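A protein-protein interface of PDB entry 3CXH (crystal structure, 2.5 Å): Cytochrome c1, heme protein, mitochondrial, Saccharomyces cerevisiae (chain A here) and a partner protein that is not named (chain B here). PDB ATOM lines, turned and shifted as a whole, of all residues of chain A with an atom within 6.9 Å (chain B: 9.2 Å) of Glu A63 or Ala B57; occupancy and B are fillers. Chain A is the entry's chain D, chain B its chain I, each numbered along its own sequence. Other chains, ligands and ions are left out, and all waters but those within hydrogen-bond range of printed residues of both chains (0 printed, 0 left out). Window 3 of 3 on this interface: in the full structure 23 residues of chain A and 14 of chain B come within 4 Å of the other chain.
NH2 of Arg A30 lies within hydrogen-bond range of O of Ser A58 (2.8 Å).
The guanidinium group (NH1) of Arg A30 is in salt-bridge range of the side-chain carboxylate (OE2) of Glu A63 (2.9 Å).
The guanidinium group (NH1) of Arg A30 is in salt-bridge range of the side-chain carboxylate (OE2) of Glu A176 (3.5 Å).
ND1 of His A59 sits at hydrogen-bond distance from OG of Ser A58.
N of Thr A60 sits at hydrogen-bond distance from OE1 of Glu A63 (3.1 Å).
Among the printed residues, merely in contact across the chains: Ser A58 with Trp B48, Arg A30 with Ala B57, Arg A30 with Trp B48, Glu A63 with Ala B57, His A59 with Trp B48, Glu A176 with Ile B55, Thr A60 with Ala B57 and Thr A60 with Trp B48.
Of chain B, only Trp B48 (3.9 Å) and Ala B57 (3.9 Å) come within 4 Å of Thr A60.
Val A64 touches none of the printed residues of chain B.
Printed residues of chain B within 4 Å of His A59: Trp B48.
Of the printed residues of chain B, Arg A30 touches Trp B48 (3.5 Å) and Ala B57 (3.4 Å).
The nearest printed residue of chain A that does not touch Trp B48 is Glu A63 (4.7 Å).
Printed residues of chain B that touch a printed residue of chain A: Trp B48, Ile B55 and Ala B57.
Hydrophobic or aromatic side chains of chain B that line the printed part of chain A: Trp B48, Ile B55 and Ala B57.
Among the printed residues, 8 pairs touch across the chains.
Among the printed residues, no Asp or Glu carboxylate lies within 4 Å of a Lys or Arg side-chain nitrogen of the other chain.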
ATOM      1  N   ARG A  30     -21.074 -14.603 -17.787  1.00  0.00           N
ATOM      2  CA  ARG A  30     -22.435 -15.138 -17.790  1.00  0.00           C
ATOM      3  C   ARG A  30     -23.394 -14.303 -16.932  1.00  0.00           C
ATOM      4  O   ARG A  30     -24.569 -14.162 -17.257  1.00  0.00           O
ATOM      5  CB  ARG A  30     -22.431 -16.584 -17.289  1.00  0.00           C
ATOM      6  CG  ARG A  30     -23.820 -17.205 -17.196  1.00  0.00           C
ATOM      7  CD  ARG A  30     -23.771 -18.643 -16.698  1.00  0.00           C
ATOM      8  NE  ARG A  30     -25.099 -19.250 -16.719  1.00  0.00           N
ATOM      9  CZ  ARG A  30     -25.540 -20.069 -17.670  1.00  0.00           C
ATOM     10  NH1 ARG A  30     -26.770 -20.559 -17.603  1.00  0.00           N
ATOM     11  NH2 ARG A  30     -24.753 -20.415 -18.679  1.00  0.00           N
ATOM     12  N   TRP A  51     -25.479 -13.522 -31.611  1.00  0.00           N
ATOM     13  CA  TRP A  51     -25.893 -14.586 -30.698  1.00  0.00           C
ATOM     14  C   TRP A  51     -24.893 -15.739 -30.648  1.00  0.00           C
ATOM     15  O   TRP A  51     -24.390 -16.064 -29.574  1.00  0.00           O
ATOM     16  CB  TRP A  51     -27.277 -15.109 -31.070  1.00  0.00           C
ATOM     17  CG  TRP A  51     -28.380 -14.135 -30.809  1.00  0.00           C
ATOM     18  CD1 TRP A  51     -29.145 -13.490 -31.742  1.00  0.00           C
ATOM     19  CD2 TRP A  51     -28.858 -13.699 -29.532  1.00  0.00           C
ATOM     20  NE1 TRP A  51     -30.065 -12.681 -31.125  1.00  0.00           N
ATOM     21  CE2 TRP A  51     -29.913 -12.790 -29.768  1.00  0.00           C
ATOM     22  CE3 TRP A  51     -28.496 -13.989 -28.209  1.00  0.00           C
ATOM     23  CZ2 TRP A  51     -30.614 -12.165 -28.727  1.00  0.00           C
ATOM     24  CZ3 TRP A  51     -29.192 -13.367 -27.175  1.00  0.00           C
ATOM     25  CH2 TRP A  51     -30.240 -12.464 -27.441  1.00  0.00           C
ATOM     26  N   VAL A  55     -22.385 -18.729 -27.452  1.00  0.00           N
ATOM     27  CA  VAL A  55     -22.274 -20.184 -27.353  1.00  0.00           C
ATOM     28  C   VAL A  55     -20.858 -20.658 -27.059  1.00  0.00           C
ATOM     29  O   VAL A  55     -19.937 -20.442 -27.858  1.00  0.00           O
ATOM     30  CB  VAL A  55     -22.742 -20.896 -28.656  1.00  0.00           C
ATOM     31  CG1 VAL A  55     -22.646 -22.409 -28.498  1.00  0.00           C
ATOM     32  CG2 VAL A  55     -24.159 -20.503 -29.014  1.00  0.00           C
ATOM     33  N   SER A  58     -20.385 -18.271 -22.406  1.00  0.00           N
ATOM     34  CA  SER A  58     -21.151 -17.961 -21.215  1.00  0.00           C
ATOM     35  C   SER A  58     -22.493 -18.690 -21.186  1.00  0.00           C
ATOM     36  O   SER A  58     -23.189 -18.672 -20.171  1.00  0.00           O
ATOM     37  CB  SER A  58     -21.374 -16.453 -21.136  1.00  0.00           C
ATOM     38  OG  SER A  58     -22.059 -15.992 -22.286  1.00  0.00           O
ATOM     39  N   HIS A  59     -22.852 -19.319 -22.303  1.00  0.00           N
ATOM     40  CA  HIS A  59     -24.107 -20.058 -22.425  1.00  0.00           C
ATOM     41  C   HIS A  59     -23.939 -21.245 -23.368  1.00  0.00           C
ATOM     42  O   HIS A  59     -23.014 -21.275 -24.181  1.00  0.00           O
ATOM     43  CB  HIS A  59     -25.223 -19.160 -22.966  1.00  0.00           C
ATOM     44  CG  HIS A  59     -25.535 -17.979 -22.099  1.00  0.00           C
ATOM     45  ND1 HIS A  59     -24.759 -16.837 -22.087  1.00  0.00           N
ATOM     46  CD2 HIS A  59     -26.547 -17.755 -21.227  1.00  0.00           C
ATOM     47  CE1 HIS A  59     -25.280 -15.963 -21.245  1.00  0.00           C
ATOM     48  NE2 HIS A  59     -26.365 -16.494 -20.711  1.00  0.00           N
ATOM     49  N   THR A  60     -24.828 -22.229 -23.243  1.00  0.00           N
ATOM     50  CA  THR A  60     -24.796 -23.409 -24.101  1.00  0.00           C
ATOM     51  C   THR A  60     -25.577 -23.086 -25.376  1.00  0.00           C
ATOM     52  O   THR A  60     -26.350 -22.121 -25.414  1.00  0.00           O
ATOM     53  CB  THR A  60     -25.464 -24.617 -23.427  1.00  0.00           C
ATOM     54  OG1 THR A  60     -26.863 -24.359 -23.280  1.00  0.00           O
ATOM     55  CG2 THR A  60     -24.854 -24.876 -22.059  1.00  0.00           C
ATOM     56  N   ASN A  61     -25.411 -23.928 -26.395  1.00  0.00           N
ATOM     57  CA  ASN A  61     -26.085 -23.734 -27.672  1.00  0.00           C
ATOM     58  C   ASN A  61     -27.592 -23.562 -27.509  1.00  0.00           C
ATOM     59  O   ASN A  61     -28.162 -22.579 -27.983  1.00  0.00           O
ATOM     60  CB  ASN A  61     -25.778 -24.902 -28.618  1.00  0.00           C
ATOM     61  CG  ASN A  61     -26.358 -24.698 -30.012  1.00  0.00           C
ATOM     62  OD1 ASN A  61     -27.556 -24.889 -30.235  1.00  0.00           O
ATOM     63  ND2 ASN A  61     -25.510 -24.298 -30.954  1.00  0.00           N
ATOM     64  N   GLU A  62     -28.222 -24.491 -26.796  1.00  0.00           N
ATOM     65  CA  GLU A  62     -29.671 -24.449 -26.581  1.00  0.00           C
ATOM     66  C   GLU A  62     -30.123 -23.205 -25.822  1.00  0.00           C
ATOM     67  O   GLU A  62     -31.193 -22.658 -26.101  1.00  0.00           O
ATOM     68  CB  GLU A  62     -30.159 -25.719 -25.876  1.00  0.00           C
ATOM     69  CG  GLU A  62     -29.860 -27.015 -26.637  1.00  0.00           C
ATOM     70  CD  GLU A  62     -28.366 -27.373 -26.686  1.00  0.00           C
ATOM     71  OE1 GLU A  62     -27.612 -26.987 -25.757  1.00  0.00           O
ATOM     72  OE2 GLU A  62     -27.945 -28.048 -27.655  1.00  0.00           O
ATOM     73  N   GLU A  63     -29.303 -22.739 -24.889  1.00  0.00           N
ATOM     74  CA  GLU A  63     -29.651 -21.547 -24.132  1.00  0.00           C
ATOM     75  C   GLU A  63     -29.706 -20.310 -25.020  1.00  0.00           C
ATOM     76  O   GLU A  63     -30.649 -19.526 -24.929  1.00  0.00           O
ATOM     77  CB  GLU A  63     -28.670 -21.325 -22.987  1.00  0.00           C
ATOM     78  CG  GLU A  63     -28.797 -22.341 -21.869  1.00  0.00           C
ATOM     79  CD  GLU A  63     -27.936 -21.987 -20.684  1.00  0.00           C
ATOM     80  OE1 GLU A  63     -26.698 -22.089 -20.801  1.00  0.00           O
ATOM     81  OE2 GLU A  63     -28.498 -21.594 -19.640  1.00  0.00           O
ATOM     82  N   VAL A  64     -28.702 -20.150 -25.884  1.00  0.00           N
ATOM     83  CA  VAL A  64     -28.644 -19.004 -26.796  1.00  0.00           C
ATOM     84  C   VAL A  64     -29.764 -19.064 -27.834  1.00  0.00           C
ATOM     85  O   VAL A  64     -30.333 -18.041 -28.213  1.00  0.00           O
ATOM     86  CB  VAL A  64     -27.293 -18.923 -27.540  1.00  0.00           C
ATOM     87  CG1 VAL A  64     -27.265 -17.689 -28.423  1.00  0.00           C
ATOM     88  CG2 VAL A  64     -26.148 -18.878 -26.556  1.00  0.00           C
ATOM     89  N   ARG A  65     -30.070 -20.269 -28.291  1.00  0.00           N
ATOM     90  CA  ARG A  65     -31.125 -20.465 -29.271  1.00  0.00           C
ATOM     91  C   ARG A  65     -32.448 -19.948 -28.691  1.00  0.00           C
ATOM     92  O   ARG A  65     -33.180 -19.222 -29.364  1.00  0.00           O
ATOM     93  CB  ARG A  65     -31.234 -21.949 -29.630  1.00  0.00           C
ATOM     94  CG  ARG A  65     -31.925 -22.234 -30.952  1.00  0.00           C
ATOM     95  CD  ARG A  65     -32.240 -23.719 -31.109  1.00  0.00           C
ATOM     96  NE  ARG A  65     -31.050 -24.561 -30.963  1.00  0.00           N
ATOM     97  CZ  ARG A  65     -30.990 -25.656 -30.202  1.00  0.00           C
ATOM     98  NH1 ARG A  65     -29.865 -26.356 -30.134  1.00  0.00           N
ATOM     99  NH2 ARG A  65     -32.051 -26.048 -29.502  1.00  0.00           N
ATOM    100  N   ASN A  66     -32.717 -20.269 -27.424  1.00  0.00           N
ATOM    101  CA  ASN A  66     -33.941 -19.827 -26.765  1.00  0.00           C
ATOM    102  C   ASN A  66     -33.999 -18.319 -26.603  1.00  0.00           C
ATOM    103  O   ASN A  66     -35.035 -17.710 -26.870  1.00  0.00           O
ATOM    104  CB  ASN A  66     -34.111 -20.496 -25.395  1.00  0.00           C
ATOM    105  CG  ASN A  66     -34.378 -21.994 -25.499  1.00  0.00           C
ATOM    106  OD1 ASN A  66     -33.873 -22.779 -24.694  1.00  0.00           O
ATOM    107  ND2 ASN A  66     -35.176 -22.396 -26.489  1.00  0.00           N
ATOM    108  N   MET A  67     -32.898 -17.720 -26.156  1.00  0.00           N
ATOM    109  CA  MET A  67     -32.835 -16.274 -25.968  1.00  0.00           C
ATOM    110  C   MET A  67     -33.046 -15.579 -27.302  1.00  0.00           C
ATOM    111  O   MET A  67     -33.756 -14.573 -27.388  1.00  0.00           O
ATOM    112  CB  MET A  67     -31.480 -15.849 -25.399  1.00  0.00           C
ATOM    113  CG  MET A  67     -31.138 -16.432 -24.044  1.00  0.00           C
ATOM    114  SD  MET A  67     -29.650 -15.677 -23.371  1.00  0.00           S
ATOM    115  CE  MET A  67     -28.403 -16.734 -24.037  1.00  0.00           C
ATOM    116  N   ALA A  68     -32.427 -16.129 -28.343  1.00  0.00           N
ATOM    117  CA  ALA A  68     -32.531 -15.571 -29.682  1.00  0.00           C
ATOM    118  C   ALA A  68     -33.956 -15.663 -30.216  1.00  0.00           C
ATOM    119  O   ALA A  68     -34.474 -14.692 -30.763  1.00  0.00           O
ATOM    120  CB  ALA A  68     -31.563 -16.272 -30.618  1.00  0.00           C
ATOM    121  N   LEU A  90     -29.274 -18.156 -34.276  1.00  0.00           N
ATOM    122  CA  LEU A  90     -27.893 -17.927 -33.861  1.00  0.00           C
ATOM    123  C   LEU A  90     -27.089 -16.957 -34.728  1.00  0.00           C
ATOM    124  O   LEU A  90     -26.207 -16.273 -34.226  1.00  0.00           O
ATOM    125  CB  LEU A  90     -27.137 -19.254 -33.719  1.00  0.00           C
ATOM    126  CG  LEU A  90     -27.611 -20.191 -32.602  1.00  0.00           C
ATOM    127  CD1 LEU A  90     -26.602 -21.300 -32.404  1.00  0.00           C
ATOM    128  CD2 LEU A  90     -27.791 -19.430 -31.307  1.00  0.00           C
ATOM    129  N   GLU A 176     -28.793 -16.249 -11.132  1.00  0.00           N
ATOM    130  CA  GLU A 176     -29.107 -17.668 -11.246  1.00  0.00           C
ATOM    131  C   GLU A 176     -28.319 -18.528 -10.250  1.00  0.00           C
ATOM    132  O   GLU A 176     -28.876 -19.435  -9.628  1.00  0.00           O
ATOM    133  CB  GLU A 176     -28.832 -18.140 -12.680  1.00  0.00           C
ATOM    134  CG  GLU A 176     -29.260 -19.577 -12.980  1.00  0.00           C
ATOM    135  CD  GLU A 176     -28.814 -20.060 -14.360  1.00  0.00           C
ATOM    136  OE1 GLU A 176     -28.130 -21.113 -14.431  1.00  0.00           O
ATOM    137  OE2 GLU A 176     -29.146 -19.390 -15.370  1.00  0.00           O
ATOM    138  N   TRP B  48     -14.957 -21.628 -19.433  1.00  0.00           N
ATOM    139  CA  TRP B  48     -16.338 -22.031 -19.651  1.00  0.00           C
ATOM    140  C   TRP B  48     -16.541 -23.487 -19.257  1.00  0.00           C
ATOM    141  O   TRP B  48     -17.532 -23.806 -18.615  1.00  0.00           O
ATOM    142  CB  TRP B  48     -16.734 -21.842 -21.113  1.00  0.00           C
ATOM    143  CG  TRP B  48     -18.062 -22.447 -21.445  1.00  0.00           C
ATOM    144  CD1 TRP B  48     -18.315 -23.411 -22.380  1.00  0.00           C
ATOM    145  CD2 TRP B  48     -19.322 -22.135 -20.839  1.00  0.00           C
ATOM    146  NE1 TRP B  48     -19.655 -23.714 -22.397  1.00  0.00           N
ATOM    147  CE2 TRP B  48     -20.297 -22.945 -21.463  1.00  0.00           C
ATOM    148  CE3 TRP B  48     -19.722 -21.250 -19.825  1.00  0.00           C
ATOM    149  CZ2 TRP B  48     -21.646 -22.898 -21.108  1.00  0.00           C
ATOM    150  CZ3 TRP B  48     -21.066 -21.206 -19.470  1.00  0.00           C
ATOM    151  CH2 TRP B  48     -22.011 -22.025 -20.112  1.00  0.00           C
ATOM    152  N   LYS B  49     -15.618 -24.359 -19.663  1.00  0.00           N
ATOM    153  CA  LYS B  49     -15.696 -25.784 -19.340  1.00  0.00           C
ATOM    154  C   LYS B  49     -15.912 -25.948 -17.848  1.00  0.00           C
ATOM    155  O   LYS B  49     -16.810 -26.664 -17.409  1.00  0.00           O
ATOM    156  CB  LYS B  49     -14.394 -26.508 -19.679  1.00  0.00           C
ATOM    157  CG  LYS B  49     -13.994 -26.520 -21.131  1.00  0.00           C
ATOM    158  CD  LYS B  49     -12.878 -27.537 -21.351  1.00  0.00           C
ATOM    159  CE  LYS B  49     -11.725 -27.341 -20.368  1.00  0.00           C
ATOM    160  NZ  LYS B  49     -10.676 -28.386 -20.550  1.00  0.00           N
ATOM    161  N   VAL B  51     -16.944 -23.712 -15.641  1.00  0.00           N
ATOM    162  CA  VAL B  51     -18.224 -23.142 -15.227  1.00  0.00           C
ATOM    163  C   VAL B  51     -19.423 -23.978 -15.701  1.00  0.00           C
ATOM    164  O   VAL B  51     -20.465 -24.009 -15.047  1.00  0.00           O
ATOM    165  CB  VAL B  51     -18.357 -21.689 -15.738  1.00  0.00           C
ATOM    166  CG1 VAL B  51     -19.703 -21.093 -15.353  1.00  0.00           C
ATOM    167  CG2 VAL B  51     -17.226 -20.839 -15.179  1.00  0.00           C
ATOM    168  N   LYS B  52     -19.256 -24.678 -16.820  1.00  0.00           N
ATOM    169  CA  LYS B  52     -20.311 -25.515 -17.395  1.00  0.00           C
ATOM    170  C   LYS B  52     -20.579 -26.786 -16.586  1.00  0.00           C
ATOM    171  O   LYS B  52     -21.719 -27.252 -16.518  1.00  0.00           O
ATOM    172  CB  LYS B  52     -19.952 -25.895 -18.832  1.00  0.00           C
ATOM    173  CG  LYS B  52     -21.028 -26.665 -19.572  1.00  0.00           C
ATOM    174  CD  LYS B  52     -20.466 -27.254 -20.852  1.00  0.00           C
ATOM    175  CE  LYS B  52     -21.507 -28.067 -21.595  1.00  0.00           C
ATOM    176  NZ  LYS B  52     -20.883 -28.820 -22.711  1.00  0.00           N
ATOM    177  N   ALA B  53     -19.522 -27.364 -16.015  1.00  0.00           N
ATOM    178  CA  ALA B  53     -19.632 -28.582 -15.209  1.00  0.00           C
ATOM    179  C   ALA B  53     -20.406 -28.285 -13.925  1.00  0.00           C
ATOM    180  O   ALA B  53     -21.421 -28.925 -13.636  1.00  0.00           O
ATOM    181  CB  ALA B  53     -18.243 -29.128 -14.879  1.00  0.00           C
ATOM    182  N   ARG B  54     -19.919 -27.299 -13.173  1.00  0.00           N
ATOM    183  CA  ARG B  54     -20.545 -26.868 -11.925  1.00  0.00           C
ATOM    184  C   ARG B  54     -21.993 -26.485 -12.229  1.00  0.00           C
ATOM    185  O   ARG B  54     -22.910 -27.287 -12.038  1.00  0.00           O
ATOM    186  CB  ARG B  54     -19.782 -25.664 -11.356  1.00  0.00           C
ATOM    187  CG  ARG B  54     -18.348 -25.979 -10.922  1.00  0.00           C
ATOM    188  CD  ARG B  54     -17.428 -24.754 -10.994  1.00  0.00           C
ATOM    189  NE  ARG B  54     -17.900 -23.621 -10.197  1.00  0.00           N
ATOM    190  CZ  ARG B  54     -17.443 -22.376 -10.315  1.00  0.00           C
ATOM    191  NH1 ARG B  54     -16.493 -22.090 -11.199  1.00  0.00           N
ATOM    192  NH2 ARG B  54     -17.942 -21.409  -9.555  1.00  0.00           N
ATOM    193  N   ILE B  55     -22.179 -25.273 -12.743  1.00  0.00           N
ATOM    194  CA  ILE B  55     -23.503 -24.778 -13.105  1.00  0.00           C
ATOM    195  C   ILE B  55     -23.937 -25.528 -14.368  1.00  0.00           C
ATOM    196  O   ILE B  55     -23.774 -25.029 -15.487  1.00  0.00           O
ATOM    197  CB  ILE B  55     -23.477 -23.245 -13.381  1.00  0.00           C
ATOM    198  CG1 ILE B  55     -22.946 -22.493 -12.155  1.00  0.00           C
ATOM    199  CG2 ILE B  55     -24.869 -22.741 -13.746  1.00  0.00           C
ATOM    200  CD1 ILE B  55     -23.770 -22.698 -10.890  1.00  0.00           C
ATOM    201  N   ALA B  56     -24.444 -26.748 -14.172  1.00  0.00           N
ATOM    202  CA  ALA B  56     -24.894 -27.605 -15.269  1.00  0.00           C
ATOM    203  C   ALA B  56     -26.140 -27.046 -15.967  1.00  0.00           C
ATOM    204  O   ALA B  56     -27.270 -27.444 -15.668  1.00  0.00           O
ATOM    205  CB  ALA B  56     -25.150 -29.022 -14.756  1.00  0.00           C
ATOM    206  N   ALA B  57     -25.911 -26.121 -16.901  1.00  0.00           N
ATOM    207  CA  ALA B  57     -26.984 -25.475 -17.660  1.00  0.00           C
ATOM    208  C   ALA B  57     -27.065 -25.978 -19.102  1.00  0.00           C
ATOM    209  O   ALA B  57     -28.030 -25.599 -19.803  1.00  0.00           O
ATOM    210  CB  ALA B  57     -26.795 -23.961 -17.638  1.00  0.00           C
